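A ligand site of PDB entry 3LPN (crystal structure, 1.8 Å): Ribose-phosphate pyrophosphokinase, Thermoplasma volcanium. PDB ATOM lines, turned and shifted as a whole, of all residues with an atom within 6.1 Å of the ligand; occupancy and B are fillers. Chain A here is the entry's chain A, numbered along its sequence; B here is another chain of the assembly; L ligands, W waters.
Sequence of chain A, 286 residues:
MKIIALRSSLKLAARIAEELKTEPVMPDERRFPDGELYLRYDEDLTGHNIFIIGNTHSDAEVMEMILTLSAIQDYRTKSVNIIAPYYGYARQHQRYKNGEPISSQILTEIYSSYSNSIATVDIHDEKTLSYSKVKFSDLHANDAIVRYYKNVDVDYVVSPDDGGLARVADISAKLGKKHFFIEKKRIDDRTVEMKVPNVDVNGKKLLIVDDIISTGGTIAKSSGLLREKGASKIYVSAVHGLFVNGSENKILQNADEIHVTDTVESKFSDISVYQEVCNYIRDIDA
OD1 of Asp 125 sits close to O3 of the ligand. The side-chain hydroxyl (OH) of Tyr 96 lies within hydrogen-bond range of an oxygen (O4) of the ligand, at 2.7 Å. The side-chain amide oxygen (OE1) of Gln 92 sits at hydrogen-bond distance from an oxygen (O12) of the ligand, at 2.7 Å. O3 of the ligand is in hydrogen-bond range of NE2 of His 93 (2.8 Å). A ring nitrogen (NE2) of His 124 is in hydrogen-bond range of an oxygen (O1) of the ligand. The side-chain carboxylate (OE1) of Glu 36 of chain B is in hydrogen-bond range of a nitrogen (N3) of the ligand. OD2 of Asp 34 of chain B lies within hydrogen-bond range of N3 of the ligand (2.9 Å).
A ring nitrogen (NE2) of His 93 sits at hydrogen-bond distance from the side-chain carboxylate (OD1) of Asp 125 (3.4 Å). The side-chain hydroxyl (OH) of Tyr 96 lies within hydrogen-bond range of a ring nitrogen (NE2) of His 93 (3.2 Å). OE1 of Glu 100 sits at hydrogen-bond distance from N of Tyr 96, 2.8 Å away. The side-chain carboxylate of Glu 100 lies within hydrogen-bond range of the side-chain amide nitrogen of Gln 92, 2.9 Å away. The backbone carbonyl oxygen (O) of Gln 94 lies within hydrogen-bond range of the side-chain amide nitrogen (NE2) of Gln 92 (3.3 Å). The backbone NH (N) of Glu 36 of chain B lies within hydrogen-bond range of the side-chain carboxylate (OD1) of Asp 34 of chain B, 3.0 Å away. N of Tyr 89 is in hydrogen-bond range of OE2 of Glu 36 of chain B. The guanidinium group (NH2) of Arg 91 lies within salt-bridge range of the side-chain carboxylate (OD2) of Asp 34 of chain B, at 2.9 Å.
Merely in contact with the ligand: Phe 32 of chain B and Arg 91. Hydrophobic or aromatic side chains within 4 Å of the ligand: His 93, Tyr 96, His 124 and Phe 32 of chain B. Nine residues have an atom within 4 Å of the ligand: Arg 91, Gln 92, His 93, Tyr 96, His 124, Asp 125, Phe 32 of chain B, Asp 34 of chain B and Glu 36 of chain B. The nearest printed residue that does not touch the ligand is Tyr 38 of chain B (4.5 Å).
Water W4 lies within hydrogen-bond range of O of Arg 91, O4 of the ligand and OH of Tyr 96. Water W1 bridges OE1 of Glu 36 of chain B (2.7 Å) and N2 of the ligand (2.9 Å). Water W3 lies within hydrogen-bond range of OE2 of Glu 100 (2.6 Å) and O12 of the ligand (2.9 Å). Water W9 lies within hydrogen-bond range of N4 of the ligand, N of Asp 34 of chain B and OG of Ser 214. Water W5 lies within hydrogen-bond range of an oxygen (O5) of the ligand and the side-chain amide oxygen of Gln 94.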
ATOM      1  N   TYR A  86      -7.604  -3.976   9.438  1.00  0.00           N
ATOM      2  CA  TYR A  86      -6.896  -5.195   9.062  1.00  0.00           C
ATOM      3  C   TYR A  86      -5.686  -4.794   8.249  1.00  0.00           C
ATOM      4  O   TYR A  86      -5.822  -4.133   7.212  1.00  0.00           O
ATOM      5  CB  TYR A  86      -7.788  -6.156   8.264  1.00  0.00           C
ATOM      6  CG  TYR A  86      -7.044  -7.394   7.816  1.00  0.00           C
ATOM      7  CD1 TYR A  86      -6.341  -8.165   8.723  1.00  0.00           C
ATOM      8  CD2 TYR A  86      -7.044  -7.793   6.480  1.00  0.00           C
ATOM      9  CE1 TYR A  86      -5.648  -9.294   8.333  1.00  0.00           C
ATOM     10  CE2 TYR A  86      -6.357  -8.918   6.074  1.00  0.00           C
ATOM     11  CZ  TYR A  86      -5.661  -9.675   6.999  1.00  0.00           C
ATOM     12  OH  TYR A  86      -4.972 -10.796   6.607  1.00  0.00           O
ATOM     13  N   TYR A  89      -0.633  -8.154   4.382  1.00  0.00           N
ATOM     14  CA  TYR A  89       0.764  -8.597   4.228  1.00  0.00           C
ATOM     15  C   TYR A  89       1.511  -8.860   5.550  1.00  0.00           C
ATOM     16  O   TYR A  89       2.722  -9.119   5.541  1.00  0.00           O
ATOM     17  CB  TYR A  89       1.534  -7.652   3.308  1.00  0.00           C
ATOM     18  CG  TYR A  89       1.039  -7.743   1.892  1.00  0.00           C
ATOM     19  CD1 TYR A  89       1.612  -8.637   0.992  1.00  0.00           C
ATOM     20  CD2 TYR A  89      -0.040  -6.984   1.467  1.00  0.00           C
ATOM     21  CE1 TYR A  89       1.157  -8.741  -0.297  1.00  0.00           C
ATOM     22  CE2 TYR A  89      -0.513  -7.088   0.165  1.00  0.00           C
ATOM     23  CZ  TYR A  89       0.087  -7.974  -0.704  1.00  0.00           C
ATOM     24  OH  TYR A  89      -0.372  -8.091  -1.995  1.00  0.00           O
ATOM     25  N   ALA A  90       0.787  -8.815   6.667  1.00  0.00           N
ATOM     26  CA  ALA A  90       1.383  -9.098   7.967  1.00  0.00           C
ATOM     27  C   ALA A  90       1.938 -10.517   8.052  1.00  0.00           C
ATOM     28  O   ALA A  90       2.796 -10.808   8.875  1.00  0.00           O
ATOM     29  CB  ALA A  90       0.369  -8.852   9.092  1.00  0.00           C
ATOM     30  N   ARG A  91       1.411 -11.395   7.208  1.00  0.00           N
ATOM     31  CA  ARG A  91       1.857 -12.790   7.177  1.00  0.00           C
ATOM     32  C   ARG A  91       3.213 -12.954   6.482  1.00  0.00           C
ATOM     33  O   ARG A  91       3.910 -13.949   6.722  1.00  0.00           O
ATOM     34  CB  ARG A  91       0.795 -13.657   6.502  1.00  0.00           C
ATOM     35  CG  ARG A  91      -0.331 -14.103   7.426  1.00  0.00           C
ATOM     36  CD  ARG A  91      -1.660 -14.120   6.700  1.00  0.00           C
ATOM     37  NE  ARG A  91      -2.334 -15.404   6.808  1.00  0.00           N
ATOM     38  CZ  ARG A  91      -3.553 -15.654   6.315  1.00  0.00           C
ATOM     39  NH1 ARG A  91      -4.084 -16.860   6.462  1.00  0.00           N
ATOM     40  NH2 ARG A  91      -4.237 -14.703   5.690  1.00  0.00           N
ATOM     41  N   GLN A  92       3.586 -11.992   5.646  1.00  0.00           N
ATOM     42  CA  GLN A  92       4.897 -12.003   5.001  1.00  0.00           C
ATOM     43  C   GLN A  92       5.804 -10.963   5.672  1.00  0.00           C
ATOM     44  O   GLN A  92       6.141  -9.932   5.079  1.00  0.00           O
ATOM     45  CB  GLN A  92       4.768 -11.735   3.496  1.00  0.00           C
ATOM     46  CG  GLN A  92       6.065 -11.952   2.698  1.00  0.00           C
ATOM     47  CD  GLN A  92       6.427 -13.423   2.521  1.00  0.00           C
ATOM     48  OE1 GLN A  92       5.599 -14.310   2.743  1.00  0.00           O
ATOM     49  NE2 GLN A  92       7.667 -13.690   2.114  1.00  0.00           N
ATOM     50  N   HIS A  93       6.205 -11.274   6.906  1.00  0.00           N
ATOM     51  CA  HIS A  93       6.944 -10.328   7.740  1.00  0.00           C
ATOM     52  C   HIS A  93       8.438 -10.650   7.790  1.00  0.00           C
ATOM     53  O   HIS A  93       9.199 -10.019   8.512  1.00  0.00           O
ATOM     54  CB  HIS A  93       6.359 -10.275   9.155  1.00  0.00           C
ATOM     55  CG  HIS A  93       6.232 -11.624   9.795  1.00  0.00           C
ATOM     56  ND1 HIS A  93       7.314 -12.315  10.294  1.00  0.00           N
ATOM     57  CD2 HIS A  93       5.151 -12.407  10.017  1.00  0.00           C
ATOM     58  CE1 HIS A  93       6.906 -13.467  10.801  1.00  0.00           C
ATOM     59  NE2 HIS A  93       5.594 -13.551  10.645  1.00  0.00           N
ATOM     60  N   GLN A  94       8.842 -11.634   6.992  1.00  0.00           N
ATOM     61  CA  GLN A  94      10.244 -11.956   6.826  1.00  0.00           C
ATOM     62  C   GLN A  94      10.400 -12.712   5.512  1.00  0.00           C
ATOM     63  O   GLN A  94       9.413 -13.026   4.842  1.00  0.00           O
ATOM     64  CB  GLN A  94      10.712 -12.846   7.973  1.00  0.00           C
ATOM     65  CG  GLN A  94      10.272 -14.289   7.808  1.00  0.00           C
ATOM     66  CD  GLN A  94      10.811 -15.180   8.894  1.00  0.00           C
ATOM     67  OE1 GLN A  94      10.511 -15.000  10.068  1.00  0.00           O
ATOM     68  NE2 GLN A  94      11.617 -16.164   8.510  1.00  0.00           N
ATOM     69  N   TYR A  96      11.019 -16.153   3.847  1.00  0.00           N
ATOM     70  CA  TYR A  96      10.963 -17.577   4.181  1.00  0.00           C
ATOM     71  C   TYR A  96      11.770 -18.426   3.203  1.00  0.00           C
ATOM     72  O   TYR A  96      12.036 -19.606   3.456  1.00  0.00           O
ATOM     73  CB  TYR A  96       9.514 -18.064   4.231  1.00  0.00           C
ATOM     74  CG  TYR A  96       8.697 -17.317   5.253  1.00  0.00           C
ATOM     75  CD1 TYR A  96       8.598 -17.761   6.573  1.00  0.00           C
ATOM     76  CD2 TYR A  96       8.035 -16.135   4.923  1.00  0.00           C
ATOM     77  CE1 TYR A  96       7.868 -17.061   7.512  1.00  0.00           C
ATOM     78  CE2 TYR A  96       7.290 -15.444   5.851  1.00  0.00           C
ATOM     79  CZ  TYR A  96       7.208 -15.911   7.147  1.00  0.00           C
ATOM     80  OH  TYR A  96       6.470 -15.197   8.067  1.00  0.00           O
ATOM     81  N   GLU A 100      12.567 -13.777  -1.660  1.00  0.00           N
ATOM     82  CA  GLU A 100      11.207 -13.361  -1.344  1.00  0.00           C
ATOM     83  C   GLU A 100      11.224 -11.921  -0.868  1.00  0.00           C
ATOM     84  O   GLU A 100      12.216 -11.461  -0.309  1.00  0.00           O
ATOM     85  CB  GLU A 100      10.619 -14.245  -0.233  1.00  0.00           C
ATOM     86  CG  GLU A 100      10.104 -15.599  -0.712  1.00  0.00           C
ATOM     87  CD  GLU A 100       9.435 -16.370   0.400  1.00  0.00           C
ATOM     88  OE1 GLU A 100       9.511 -15.906   1.555  1.00  0.00           O
ATOM     89  OE2 GLU A 100       8.847 -17.444   0.133  1.00  0.00           O
ATOM     90  N   HIS A 124      -1.038  -9.622  12.607  1.00  0.00           N
ATOM     91  CA  HIS A 124      -0.457 -10.947  12.673  1.00  0.00           C
ATOM     92  C   HIS A 124       1.052 -10.848  12.847  1.00  0.00           C
ATOM     93  O   HIS A 124       1.785 -10.533  11.914  1.00  0.00           O
ATOM     94  CB  HIS A 124      -0.783 -11.779  11.430  1.00  0.00           C
ATOM     95  CG  HIS A 124      -0.352 -13.212  11.549  1.00  0.00           C
ATOM     96  ND1 HIS A 124      -1.141 -14.168  12.159  1.00  0.00           N
ATOM     97  CD2 HIS A 124       0.793 -13.831  11.205  1.00  0.00           C
ATOM     98  CE1 HIS A 124      -0.500 -15.325  12.152  1.00  0.00           C
ATOM     99  NE2 HIS A 124       0.673 -15.145  11.577  1.00  0.00           N
ATOM    100  N   ASP A 125       1.513 -11.116  14.074  1.00  0.00           N
ATOM    101  CA  ASP A 125       2.928 -11.036  14.416  1.00  0.00           C
ATOM    102  C   ASP A 125       3.455  -9.600  14.483  1.00  0.00           C
ATOM    103  O   ASP A 125       3.501  -8.893  13.477  1.00  0.00           O
ATOM    104  CB  ASP A 125       3.788 -11.869  13.463  1.00  0.00           C
ATOM    105  CG  ASP A 125       5.164 -12.166  14.043  1.00  0.00           C
ATOM    106  OD1 ASP A 125       5.577 -13.342  14.009  1.00  0.00           O
ATOM    107  OD2 ASP A 125       5.822 -11.235  14.561  1.00  0.00           O
ATOM    108  N   SER A 214      -9.075 -17.195   6.973  1.00  0.00           N
ATOM    109  CA  SER A 214      -8.919 -17.088   5.529  1.00  0.00           C
ATOM    110  C   SER A 214      -9.676 -18.233   4.870  1.00  0.00           C
ATOM    111  O   SER A 214     -10.864 -18.089   4.576  1.00  0.00           O
ATOM    112  CB  SER A 214      -7.436 -17.118   5.157  1.00  0.00           C
ATOM    113  OG  SER A 214      -7.247 -16.814   3.770  1.00  0.00           O
ATOM    114  N   ARG B  30       2.468 -15.880  -7.628  1.00  0.00           N
ATOM    115  CA  ARG B  30       1.155 -16.467  -7.417  1.00  0.00           C
ATOM    116  C   ARG B  30       0.362 -15.631  -6.428  1.00  0.00           C
ATOM    117  O   ARG B  30       0.910 -14.737  -5.780  1.00  0.00           O
ATOM    118  CB  ARG B  30       1.295 -17.906  -6.903  1.00  0.00           C
ATOM    119  CG  ARG B  30       2.026 -17.994  -5.572  1.00  0.00           C
ATOM    120  CD  ARG B  30       2.315 -19.432  -5.172  1.00  0.00           C
ATOM    121  NE  ARG B  30       3.308 -19.496  -4.096  1.00  0.00           N
ATOM    122  CZ  ARG B  30       3.024 -19.664  -2.805  1.00  0.00           C
ATOM    123  NH1 ARG B  30       1.757 -19.804  -2.422  1.00  0.00           N
ATOM    124  NH2 ARG B  30       3.994 -19.693  -1.919  1.00  0.00           N
ATOM    125  N   PHE B  32      -1.889 -15.760  -2.956  1.00  0.00           N
ATOM    126  CA  PHE B  32      -2.370 -16.526  -1.807  1.00  0.00           C
ATOM    127  C   PHE B  32      -3.881 -16.597  -1.885  1.00  0.00           C
ATOM    128  O   PHE B  32      -4.517 -15.808  -2.595  1.00  0.00           O
ATOM    129  CB  PHE B  32      -1.925 -15.870  -0.487  1.00  0.00           C
ATOM    130  CG  PHE B  32      -0.444 -15.976  -0.217  1.00  0.00           C
ATOM    131  CD1 PHE B  32       0.140 -17.201   0.069  1.00  0.00           C
ATOM    132  CD2 PHE B  32       0.351 -14.841  -0.197  1.00  0.00           C
ATOM    133  CE1 PHE B  32       1.502 -17.300   0.328  1.00  0.00           C
ATOM    134  CE2 PHE B  32       1.704 -14.930   0.066  1.00  0.00           C
ATOM    135  CZ  PHE B  32       2.282 -16.151   0.337  1.00  0.00           C
ATOM    136  N   PRO B  33      -4.483 -17.556  -1.153  1.00  0.00           N
ATOM    137  CA  PRO B  33      -5.937 -17.726  -1.113  1.00  0.00           C
ATOM    138  C   PRO B  33      -6.694 -16.421  -0.799  1.00  0.00           C
ATOM    139  O   PRO B  33      -7.775 -16.209  -1.338  1.00  0.00           O
ATOM    140  CB  PRO B  33      -6.130 -18.742   0.014  1.00  0.00           C
ATOM    141  CG  PRO B  33      -4.884 -19.566  -0.030  1.00  0.00           C
ATOM    142  CD  PRO B  33      -3.784 -18.587  -0.367  1.00  0.00           C
ATOM    143  N   ASP B  34      -6.119 -15.566   0.055  1.00  0.00           N
ATOM    144  CA  ASP B  34      -6.765 -14.317   0.413  1.00  0.00           C
ATOM    145  C   ASP B  34      -6.504 -13.194  -0.593  1.00  0.00           C
ATOM    146  O   ASP B  34      -6.891 -12.040  -0.366  1.00  0.00           O
ATOM    147  CB  ASP B  34      -6.342 -13.867   1.820  1.00  0.00           C
ATOM    148  CG  ASP B  34      -4.857 -13.576   1.924  1.00  0.00           C
ATOM    149  OD1 ASP B  34      -4.182 -13.542   0.869  1.00  0.00           O
ATOM    150  OD2 ASP B  34      -4.369 -13.392   3.062  1.00  0.00           O
ATOM    151  N   GLU B  36      -3.582 -11.904  -1.606  1.00  0.00           N
ATOM    152  CA  GLU B  36      -2.294 -11.211  -1.505  1.00  0.00           C
ATOM    153  C   GLU B  36      -1.260 -11.792  -2.473  1.00  0.00           C
ATOM    154  O   GLU B  36      -1.301 -12.965  -2.811  1.00  0.00           O
ATOM    155  CB  GLU B  36      -1.759 -11.232  -0.069  1.00  0.00           C
ATOM    156  CG  GLU B  36      -2.610 -10.408   0.878  1.00  0.00           C
ATOM    157  CD  GLU B  36      -1.997 -10.239   2.255  1.00  0.00           C
ATOM    158  OE1 GLU B  36      -0.936 -10.847   2.540  1.00  0.00           O
ATOM    159  OE2 GLU B  36      -2.569  -9.484   3.060  1.00  0.00           O
ATOM    160  N   TYR B  38       2.296 -13.022  -3.950  1.00  0.00           N
ATOM    161  CA  TYR B  38       3.569 -13.646  -3.622  1.00  0.00           C
ATOM    162  C   TYR B  38       4.512 -13.574  -4.818  1.00  0.00           C
ATOM    163  O   TYR B  38       4.103 -13.857  -5.946  1.00  0.00           O
ATOM    164  CB  TYR B  38       3.352 -15.111  -3.255  1.00  0.00           C
ATOM    165  CG  TYR B  38       4.649 -15.857  -2.994  1.00  0.00           C
ATOM    166  CD1 TYR B  38       5.253 -15.818  -1.744  1.00  0.00           C
ATOM    167  CD2 TYR B  38       5.284 -16.570  -4.001  1.00  0.00           C
ATOM    168  CE1 TYR B  38       6.446 -16.487  -1.498  1.00  0.00           C
ATOM    169  CE2 TYR B  38       6.465 -17.238  -3.775  1.00  0.00           C
ATOM    170  CZ  TYR B  38       7.049 -17.186  -2.528  1.00  0.00           C
ATOM    171  OH  TYR B  38       8.240 -17.859  -2.295  1.00  0.00           O
HETATM  172  P1  LIG L   1       3.800 -16.364  12.887  1.00  0.00           P
HETATM  173  O1  LIG L   1       2.690 -16.994  12.061  1.00  0.00           O
HETATM  174  O2  LIG L   1       3.612 -16.604  14.372  1.00  0.00           O
HETATM  175  O3  LIG L   1       4.132 -14.942  12.529  1.00  0.00           O
HETATM  176  P2  LIG L   1       5.535 -17.645  11.020  1.00  0.00           P
HETATM  177  O4  LIG L   1       5.302 -16.430  10.136  1.00  0.00           O
HETATM  178  O5  LIG L   1       6.923 -18.233  11.060  1.00  0.00           O
HETATM  179  O6  LIG L   1       5.111 -17.245  12.531  1.00  0.00           O
HETATM  180  P3  LIG L   1       4.886 -19.884   9.093  1.00  0.00           P
HETATM  181  O7  LIG L   1       6.217 -20.514   9.401  1.00  0.00           O
HETATM  182  O8  LIG L   1       3.743 -20.792   8.718  1.00  0.00           O
HETATM  183  C1  LIG L   1       4.350 -18.928  10.524  1.00  0.00           C
HETATM  184  O9  LIG L   1       5.172 -18.915   7.836  1.00  0.00           O
HETATM  185  C2  LIG L   1       4.135 -18.126   7.268  1.00  0.00           C
HETATM  186  C3  LIG L   1       3.995 -18.551   5.806  1.00  0.00           C
HETATM  187  O10 LIG L   1       2.809 -17.970   5.258  1.00  0.00           O
HETATM  188  C4  LIG L   1       5.170 -18.141   4.919  1.00  0.00           C
HETATM  189  O11 LIG L   1       5.527 -19.223   4.040  1.00  0.00           O
HETATM  190  C5  LIG L   1       4.609 -17.024   4.059  1.00  0.00           C
HETATM  191  O12 LIG L   1       5.209 -16.968   2.764  1.00  0.00           O
HETATM  192  C6  LIG L   1       3.144 -17.414   3.971  1.00  0.00           C
HETATM  193  N1  LIG L   1       2.283 -16.259   3.695  1.00  0.00           N
HETATM  194  C7  LIG L   1       2.656 -14.974   3.568  1.00  0.00           C
HETATM  195  N2  LIG L   1       1.583 -14.179   3.294  1.00  0.00           N
HETATM  196  C8  LIG L   1       0.505 -14.982   3.260  1.00  0.00           C
HETATM  197  C9  LIG L   1      -0.944 -14.810   3.024  1.00  0.00           C
HETATM  198  N3  LIG L   1      -1.462 -13.590   2.785  1.00  0.00           N
HETATM  199  N4  LIG L   1      -1.728 -15.909   3.073  1.00  0.00           N
HETATM  200  C10 LIG L   1      -1.229 -17.133   3.324  1.00  0.00           C
HETATM  201  N5  LIG L   1       0.083 -17.366   3.536  1.00  0.00           N
HETATM  202  C11 LIG L   1       0.975 -16.349   3.517  1.00  0.00           C
HETATM  203  O   HOH W   1       1.565 -11.707   1.873  1.00  0.00           O
HETATM  204  O   HOH W   2       1.134 -19.164  12.389  1.00  0.00           O
HETATM  205  O   HOH W   3       7.127 -18.708   1.545  1.00  0.00           O
HETATM  206  O   HOH W   4       3.080 -15.407   8.830  1.00  0.00           O
HETATM  207  O   HOH W   5       8.342 -15.875  12.246  1.00  0.00           O
HETATM  208  O   HOH W   6       7.233 -21.038   5.297  1.00  0.00           O
HETATM  209  O   HOH W   7       0.307 -18.902   6.666  1.00  0.00           O
HETATM  210  O   HOH W   8       3.542 -20.549   2.609  1.00  0.00           O
HETATM  211  O   HOH W   9      -4.395 -16.775   2.275  1.00  0.00           O
